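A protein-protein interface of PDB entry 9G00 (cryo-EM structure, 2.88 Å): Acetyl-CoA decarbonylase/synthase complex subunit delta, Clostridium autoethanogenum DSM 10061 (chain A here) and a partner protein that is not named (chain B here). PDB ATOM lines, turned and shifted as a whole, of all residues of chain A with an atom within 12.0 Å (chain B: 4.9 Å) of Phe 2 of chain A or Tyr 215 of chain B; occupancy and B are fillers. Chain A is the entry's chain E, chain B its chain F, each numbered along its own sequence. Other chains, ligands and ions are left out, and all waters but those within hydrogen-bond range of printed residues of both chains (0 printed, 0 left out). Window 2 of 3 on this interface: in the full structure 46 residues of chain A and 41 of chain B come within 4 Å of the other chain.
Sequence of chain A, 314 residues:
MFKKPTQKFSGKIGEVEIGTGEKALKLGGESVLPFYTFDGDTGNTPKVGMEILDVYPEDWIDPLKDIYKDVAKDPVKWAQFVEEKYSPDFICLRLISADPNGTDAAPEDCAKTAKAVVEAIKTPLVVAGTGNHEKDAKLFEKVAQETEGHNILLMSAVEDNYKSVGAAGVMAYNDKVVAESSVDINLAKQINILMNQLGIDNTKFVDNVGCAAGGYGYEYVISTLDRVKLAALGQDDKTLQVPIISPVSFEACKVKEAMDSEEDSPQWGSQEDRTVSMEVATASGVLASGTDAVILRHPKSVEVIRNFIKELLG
Phe 2 of chain A touches just these residues of chain B: Leu 211 (3.6 Å), Glu 212 (3.7 Å), Tyr 215 (3.4 Å) and Ile 251 (3.5 Å). Tyr 215 of chain B touches just one residue of chain A: Phe 2 (3.4 Å). Leu 211 of chain B touches two residues of chain A. Glu 212 of chain B touches one residue of chain A. No residue of chain A comes within 4 Å of Ala 213 of chain B. No residue of chain A comes within 4 Å of Leu 214 of chain B. No residue of chain A comes within 4 Å of Leu 217 of chain B. Of chain A, only Phe 2 (3.5 Å), Lys 3 (3.8 Å) and Pro 5 (3.6 Å) come within 4 Å of Ile 251 of chain B. No residue of chain A comes within 4 Å of Asp 257 of chain B. No residue of chain A comes within 4 Å of Thr 259 of chain B. No residue of chain A comes within 4 Å of Phe 260 of chain B. Printed residues of chain B within 4 Å of Lys 4 of chain A: Leu 211. Of the printed residues of chain B, Lys 3 of chain A touches Ile 251. Printed residues of chain B within 4 Å of Pro 5 of chain A: Ile 251.
Of the 13 printed residues of chain B, 4 touch a printed residue of chain A. Hydrophobic or aromatic side chains of chain A within 4 Å of the printed part of chain B: Phe 2 and Pro 5. Among the printed residues, no Asp or Glu carboxylate lies within 4 Å of a Lys or Arg side-chain nitrogen of the other chain.
O of Lys 4 of chain A is in hydrogen-bond range of OG1 of Thr 6 of chain A, 3.4 Å away. The side-chain hydroxyl (OH) of Tyr 215 of chain B is in hydrogen-bond range of the side-chain carboxylate (OD2) of Asp 257 of chain B (2.6 Å). OH of Tyr 215 of chain B sits at hydrogen-bond distance from OG1 of Thr 259 of chain B (3.5 Å). The backbone carbonyl oxygen (O) of Ile 251 of chain B is in hydrogen-bond range of the backbone NH (N) of Asp 257 of chain B (3.4 Å).
Among the printed residues, pairs that only touch across the chains: Phe 2 of chain A with Tyr 215 of chain B (3.4 Å), Lys 4 of chain A with Leu 211 of chain B (3.5 Å), Phe 2 of chain A with Ile 251 of chain B (3.5 Å), Pro 5 of chain A with Ile 251 of chain B (3.6 Å), Phe 2 of chain A with Leu 211 of chain B (3.6 Å), Phe 2 of chain A with Glu 212 of chain B (3.7 Å) and Lys 3 of chain A with Ile 251 of chain B (3.8 Å).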
ATOM      1  N   PHE A   2      11.035 -16.556  -9.150  1.00  0.00           N
ATOM      2  CA  PHE A   2      11.023 -18.045  -9.161  1.00  0.00           C
ATOM      3  C   PHE A   2      12.316 -18.598  -8.583  1.00  0.00           C
ATOM      4  O   PHE A   2      13.155 -17.850  -8.084  1.00  0.00           O
ATOM      5  CB  PHE A   2      10.819 -18.570 -10.586  1.00  0.00           C
ATOM      6  CG  PHE A   2      11.811 -18.036 -11.581  1.00  0.00           C
ATOM      7  CD1 PHE A   2      13.063 -18.606 -11.710  1.00  0.00           C
ATOM      8  CD2 PHE A   2      11.484 -16.969 -12.394  1.00  0.00           C
ATOM      9  CE1 PHE A   2      13.968 -18.114 -12.626  1.00  0.00           C
ATOM     10  CE2 PHE A   2      12.385 -16.480 -13.310  1.00  0.00           C
ATOM     11  CZ  PHE A   2      13.627 -17.052 -13.426  1.00  0.00           C
ATOM     12  N   LYS A   3      12.466 -19.916  -8.652  1.00  0.00           N
ATOM     13  CA  LYS A   3      13.678 -20.603  -8.228  1.00  0.00           C
ATOM     14  C   LYS A   3      14.342 -21.199  -9.461  1.00  0.00           C
ATOM     15  O   LYS A   3      13.717 -21.977 -10.191  1.00  0.00           O
ATOM     16  CB  LYS A   3      13.357 -21.695  -7.208  1.00  0.00           C
ATOM     17  CG  LYS A   3      14.564 -22.522  -6.781  1.00  0.00           C
ATOM     18  CD  LYS A   3      14.174 -23.670  -5.863  1.00  0.00           C
ATOM     19  CE  LYS A   3      13.312 -24.701  -6.580  1.00  0.00           C
ATOM     20  NZ  LYS A   3      12.993 -25.878  -5.725  1.00  0.00           N
ATOM     21  N   LYS A   4      15.597 -20.840  -9.689  1.00  0.00           N
ATOM     22  CA  LYS A   4      16.320 -21.388 -10.826  1.00  0.00           C
ATOM     23  C   LYS A   4      16.502 -22.889 -10.628  1.00  0.00           C
ATOM     24  O   LYS A   4      16.884 -23.320  -9.534  1.00  0.00           O
ATOM     25  CB  LYS A   4      17.676 -20.706 -10.978  1.00  0.00           C
ATOM     26  CG  LYS A   4      18.119 -20.509 -12.419  1.00  0.00           C
ATOM     27  CD  LYS A   4      17.266 -19.458 -13.120  1.00  0.00           C
ATOM     28  CE  LYS A   4      17.845 -19.063 -14.468  1.00  0.00           C
ATOM     29  NZ  LYS A   4      17.082 -17.947 -15.092  1.00  0.00           N
ATOM     30  N   PRO A   5      16.229 -23.719 -11.639  1.00  0.00           N
ATOM     31  CA  PRO A   5      16.386 -25.166 -11.449  1.00  0.00           C
ATOM     32  C   PRO A   5      17.825 -25.559 -11.159  1.00  0.00           C
ATOM     33  O   PRO A   5      18.698 -25.424 -12.022  1.00  0.00           O
ATOM     34  CB  PRO A   5      15.898 -25.754 -12.779  1.00  0.00           C
ATOM     35  CG  PRO A   5      15.049 -24.698 -13.381  1.00  0.00           C
ATOM     36  CD  PRO A   5      15.662 -23.403 -12.960  1.00  0.00           C
ATOM     37  N   THR A   6      18.081 -26.045  -9.946  1.00  0.00           N
ATOM     38  CA  THR A   6      19.410 -26.496  -9.534  1.00  0.00           C
ATOM     39  C   THR A   6      19.447 -28.011  -9.699  1.00  0.00           C
ATOM     40  O   THR A   6      19.139 -28.764  -8.774  1.00  0.00           O
ATOM     41  CB  THR A   6      19.710 -26.086  -8.095  1.00  0.00           C
ATOM     42  OG1 THR A   6      19.528 -24.671  -7.945  1.00  0.00           O
ATOM     43  CG2 THR A   6      21.142 -26.447  -7.723  1.00  0.00           C
ATOM     44  N   GLN A   7      19.825 -28.461 -10.893  1.00  0.00           N
ATOM     45  CA  GLN A   7      19.896 -29.883 -11.210  1.00  0.00           C
ATOM     46  C   GLN A   7      21.336 -30.345 -11.030  1.00  0.00           C
ATOM     47  O   GLN A   7      22.213 -29.988 -11.824  1.00  0.00           O
ATOM     48  CB  GLN A   7      19.412 -30.150 -12.633  1.00  0.00           C
ATOM     49  CG  GLN A   7      19.283 -31.630 -12.968  1.00  0.00           C
ATOM     50  CD  GLN A   7      18.707 -31.869 -14.350  1.00  0.00           C
ATOM     51  OE1 GLN A   7      18.926 -31.084 -15.272  1.00  0.00           O
ATOM     52  NE2 GLN A   7      17.959 -32.958 -14.499  1.00  0.00           N
ATOM     53  N   PHE A  38      23.810 -23.861 -19.129  1.00  0.00           N
ATOM     54  CA  PHE A  38      23.272 -23.179 -17.961  1.00  0.00           C
ATOM     55  C   PHE A  38      23.213 -24.071 -16.726  1.00  0.00           C
ATOM     56  O   PHE A  38      23.025 -23.552 -15.621  1.00  0.00           O
ATOM     57  CB  PHE A  38      21.872 -22.636 -18.267  1.00  0.00           C
ATOM     58  CG  PHE A  38      20.965 -23.623 -18.950  1.00  0.00           C
ATOM     59  CD1 PHE A  38      20.915 -23.700 -20.331  1.00  0.00           C
ATOM     60  CD2 PHE A  38      20.152 -24.460 -18.214  1.00  0.00           C
ATOM     61  CE1 PHE A  38      20.086 -24.598 -20.956  1.00  0.00           C
ATOM     62  CE2 PHE A  38      19.320 -25.357 -18.840  1.00  0.00           C
ATOM     63  CZ  PHE A  38      19.287 -25.424 -20.212  1.00  0.00           C
ATOM     64  N   ASP A  39      23.362 -25.386 -16.883  1.00  0.00           N
ATOM     65  CA  ASP A  39      23.343 -26.302 -15.749  1.00  0.00           C
ATOM     66  C   ASP A  39      24.727 -26.592 -15.192  1.00  0.00           C
ATOM     67  O   ASP A  39      24.868 -26.785 -13.979  1.00  0.00           O
ATOM     68  CB  ASP A  39      22.707 -27.633 -16.147  1.00  0.00           C
ATOM     69  CG  ASP A  39      21.240 -27.703 -15.818  1.00  0.00           C
ATOM     70  OD1 ASP A  39      20.670 -26.678 -15.388  1.00  0.00           O
ATOM     71  OD2 ASP A  39      20.653 -28.791 -15.982  1.00  0.00           O
ATOM     72  N   LEU B 211      13.787 -14.168 -18.229  1.00  0.00           N
ATOM     73  CA  LEU B 211      12.861 -15.016 -17.485  1.00  0.00           C
ATOM     74  C   LEU B 211      12.281 -14.286 -16.281  1.00  0.00           C
ATOM     75  O   LEU B 211      11.094 -14.437 -15.974  1.00  0.00           O
ATOM     76  CB  LEU B 211      13.557 -16.301 -17.044  1.00  0.00           C
ATOM     77  CG  LEU B 211      13.899 -17.286 -18.160  1.00  0.00           C
ATOM     78  CD1 LEU B 211      14.721 -18.430 -17.609  1.00  0.00           C
ATOM     79  CD2 LEU B 211      12.641 -17.809 -18.826  1.00  0.00           C
ATOM     80  N   GLU B 212      13.101 -13.506 -15.572  1.00  0.00           N
ATOM     81  CA  GLU B 212      12.591 -12.783 -14.413  1.00  0.00           C
ATOM     82  C   GLU B 212      11.511 -11.790 -14.821  1.00  0.00           C
ATOM     83  O   GLU B 212      10.474 -11.682 -14.157  1.00  0.00           O
ATOM     84  CB  GLU B 212      13.724 -12.061 -13.688  1.00  0.00           C
ATOM     85  CG  GLU B 212      14.501 -12.931 -12.714  1.00  0.00           C
ATOM     86  CD  GLU B 212      15.509 -13.828 -13.401  1.00  0.00           C
ATOM     87  OE1 GLU B 212      15.491 -13.906 -14.648  1.00  0.00           O
ATOM     88  OE2 GLU B 212      16.327 -14.450 -12.692  1.00  0.00           O
ATOM     89  N   ALA B 213      11.736 -11.051 -15.908  1.00  0.00           N
ATOM     90  CA  ALA B 213      10.711 -10.134 -16.391  1.00  0.00           C
ATOM     91  C   ALA B 213       9.486 -10.894 -16.883  1.00  0.00           C
ATOM     92  O   ALA B 213       8.350 -10.474 -16.642  1.00  0.00           O
ATOM     93  CB  ALA B 213      11.277  -9.251 -17.500  1.00  0.00           C
ATOM     94  N   LEU B 214       9.698 -12.011 -17.579  1.00  0.00           N
ATOM     95  CA  LEU B 214       8.571 -12.817 -18.033  1.00  0.00           C
ATOM     96  C   LEU B 214       7.804 -13.400 -16.855  1.00  0.00           C
ATOM     97  O   LEU B 214       6.570 -13.407 -16.854  1.00  0.00           O
ATOM     98  CB  LEU B 214       9.059 -13.931 -18.958  1.00  0.00           C
ATOM     99  CG  LEU B 214       7.974 -14.829 -19.557  1.00  0.00           C
ATOM    100  CD1 LEU B 214       7.012 -14.026 -20.411  1.00  0.00           C
ATOM    101  CD2 LEU B 214       8.603 -15.935 -20.372  1.00  0.00           C
ATOM    102  N   TYR B 215       8.517 -13.895 -15.844  1.00  0.00           N
ATOM    103  CA  TYR B 215       7.842 -14.478 -14.690  1.00  0.00           C
ATOM    104  C   TYR B 215       6.998 -13.440 -13.964  1.00  0.00           C
ATOM    105  O   TYR B 215       5.865 -13.722 -13.562  1.00  0.00           O
ATOM    106  CB  TYR B 215       8.863 -15.088 -13.737  1.00  0.00           C
ATOM    107  CG  TYR B 215       8.245 -15.911 -12.637  1.00  0.00           C
ATOM    108  CD1 TYR B 215       7.963 -17.252 -12.830  1.00  0.00           C
ATOM    109  CD2 TYR B 215       7.950 -15.349 -11.405  1.00  0.00           C
ATOM    110  CE1 TYR B 215       7.402 -18.013 -11.830  1.00  0.00           C
ATOM    111  CE2 TYR B 215       7.387 -16.103 -10.396  1.00  0.00           C
ATOM    112  CZ  TYR B 215       7.117 -17.434 -10.615  1.00  0.00           C
ATOM    113  OH  TYR B 215       6.557 -18.193  -9.615  1.00  0.00           O
ATOM    114  N   GLY B 216       7.535 -12.234 -13.786  1.00  0.00           N
ATOM    115  CA  GLY B 216       6.765 -11.185 -13.141  1.00  0.00           C
ATOM    116  C   GLY B 216       5.569 -10.752 -13.965  1.00  0.00           C
ATOM    117  O   GLY B 216       4.506 -10.452 -13.419  1.00  0.00           O
ATOM    118  N   LEU B 217       5.727 -10.707 -15.289  1.00  0.00           N
ATOM    119  CA  LEU B 217       4.642 -10.242 -16.148  1.00  0.00           C
ATOM    120  C   LEU B 217       3.484 -11.231 -16.170  1.00  0.00           C
ATOM    121  O   LEU B 217       2.319 -10.825 -16.237  1.00  0.00           O
ATOM    122  CB  LEU B 217       5.160  -9.991 -17.563  1.00  0.00           C
ATOM    123  CG  LEU B 217       4.124  -9.452 -18.553  1.00  0.00           C
ATOM    124  CD1 LEU B 217       3.473  -8.183 -18.029  1.00  0.00           C
ATOM    125  CD2 LEU B 217       4.769  -9.194 -19.898  1.00  0.00           C
ATOM    126  N   VAL B 218       3.778 -12.533 -16.136  1.00  0.00           N
ATOM    127  CA  VAL B 218       2.706 -13.525 -16.125  1.00  0.00           C
ATOM    128  C   VAL B 218       1.896 -13.408 -14.842  1.00  0.00           C
ATOM    129  O   VAL B 218       0.681 -13.630 -14.842  1.00  0.00           O
ATOM    130  CB  VAL B 218       3.272 -14.946 -16.314  1.00  0.00           C
ATOM    131  CG1 VAL B 218       2.159 -15.976 -16.233  1.00  0.00           C
ATOM    132  CG2 VAL B 218       3.969 -15.063 -17.649  1.00  0.00           C
ATOM    133  N   GLU B 219       2.552 -13.076 -13.730  1.00  0.00           N
ATOM    134  CA  GLU B 219       1.834 -12.906 -12.471  1.00  0.00           C
ATOM    135  C   GLU B 219       0.832 -11.760 -12.556  1.00  0.00           C
ATOM    136  O   GLU B 219      -0.272 -11.853 -12.011  1.00  0.00           O
ATOM    137  CB  GLU B 219       2.819 -12.675 -11.332  1.00  0.00           C
ATOM    138  CG  GLU B 219       3.622 -13.899 -10.973  1.00  0.00           C
ATOM    139  CD  GLU B 219       4.696 -13.600  -9.953  1.00  0.00           C
ATOM    140  OE1 GLU B 219       5.145 -12.437  -9.890  1.00  0.00           O
ATOM    141  OE2 GLU B 219       5.087 -14.523  -9.212  1.00  0.00           O
ATOM    142  N   ILE B 251      11.194 -25.288 -14.672  1.00  0.00           N
ATOM    143  CA  ILE B 251      10.612 -24.592 -13.528  1.00  0.00           C
ATOM    144  C   ILE B 251       9.180 -25.055 -13.308  1.00  0.00           C
ATOM    145  O   ILE B 251       8.751 -25.279 -12.171  1.00  0.00           O
ATOM    146  CB  ILE B 251      10.688 -23.068 -13.737  1.00  0.00           C
ATOM    147  CG1 ILE B 251      12.139 -22.600 -13.637  1.00  0.00           C
ATOM    148  CG2 ILE B 251       9.823 -22.337 -12.717  1.00  0.00           C
ATOM    149  CD1 ILE B 251      12.353 -21.170 -14.058  1.00  0.00           C
ATOM    150  N   ASP B 257       5.842 -25.209 -10.368  1.00  0.00           N
ATOM    151  CA  ASP B 257       5.394 -23.824 -10.415  1.00  0.00           C
ATOM    152  C   ASP B 257       4.371 -23.684 -11.533  1.00  0.00           C
ATOM    153  O   ASP B 257       4.671 -23.986 -12.692  1.00  0.00           O
ATOM    154  CB  ASP B 257       6.575 -22.884 -10.651  1.00  0.00           C
ATOM    155  CG  ASP B 257       6.236 -21.441 -10.363  1.00  0.00           C
ATOM    156  OD1 ASP B 257       5.044 -21.082 -10.443  1.00  0.00           O
ATOM    157  OD2 ASP B 257       7.163 -20.662 -10.055  1.00  0.00           O
ATOM    158  N   THR B 259       2.977 -20.819 -12.459  1.00  0.00           N
ATOM    159  CA  THR B 259       3.094 -19.555 -13.174  1.00  0.00           C
ATOM    160  C   THR B 259       3.676 -19.767 -14.564  1.00  0.00           C
ATOM    161  O   THR B 259       3.314 -19.059 -15.510  1.00  0.00           O
ATOM    162  CB  THR B 259       3.964 -18.581 -12.380  1.00  0.00           C
ATOM    163  OG1 THR B 259       3.412 -18.402 -11.071  1.00  0.00           O
ATOM    164  CG2 THR B 259       4.046 -17.234 -13.082  1.00  0.00           C
ATOM    165  N   PHE B 260       4.593 -20.720 -14.703  1.00  0.00           N
ATOM    166  CA  PHE B 260       5.198 -21.046 -15.986  1.00  0.00           C
ATOM    167  C   PHE B 260       4.554 -22.254 -16.648  1.00  0.00           C
ATOM    168  O   PHE B 260       5.098 -22.775 -17.625  1.00  0.00           O
ATOM    169  CB  PHE B 260       6.701 -21.289 -15.816  1.00  0.00           C
ATOM    170  CG  PHE B 260       7.558 -20.051 -15.960  1.00  0.00           C
ATOM    171  CD1 PHE B 260       7.072 -18.882 -16.524  1.00  0.00           C
ATOM    172  CD2 PHE B 260       8.871 -20.076 -15.542  1.00  0.00           C
ATOM    173  CE1 PHE B 260       7.873 -17.779 -16.651  1.00  0.00           C
ATOM    174  CE2 PHE B 260       9.670 -18.971 -15.672  1.00  0.00           C
ATOM    175  CZ  PHE B 260       9.170 -17.823 -16.225  1.00  0.00           C
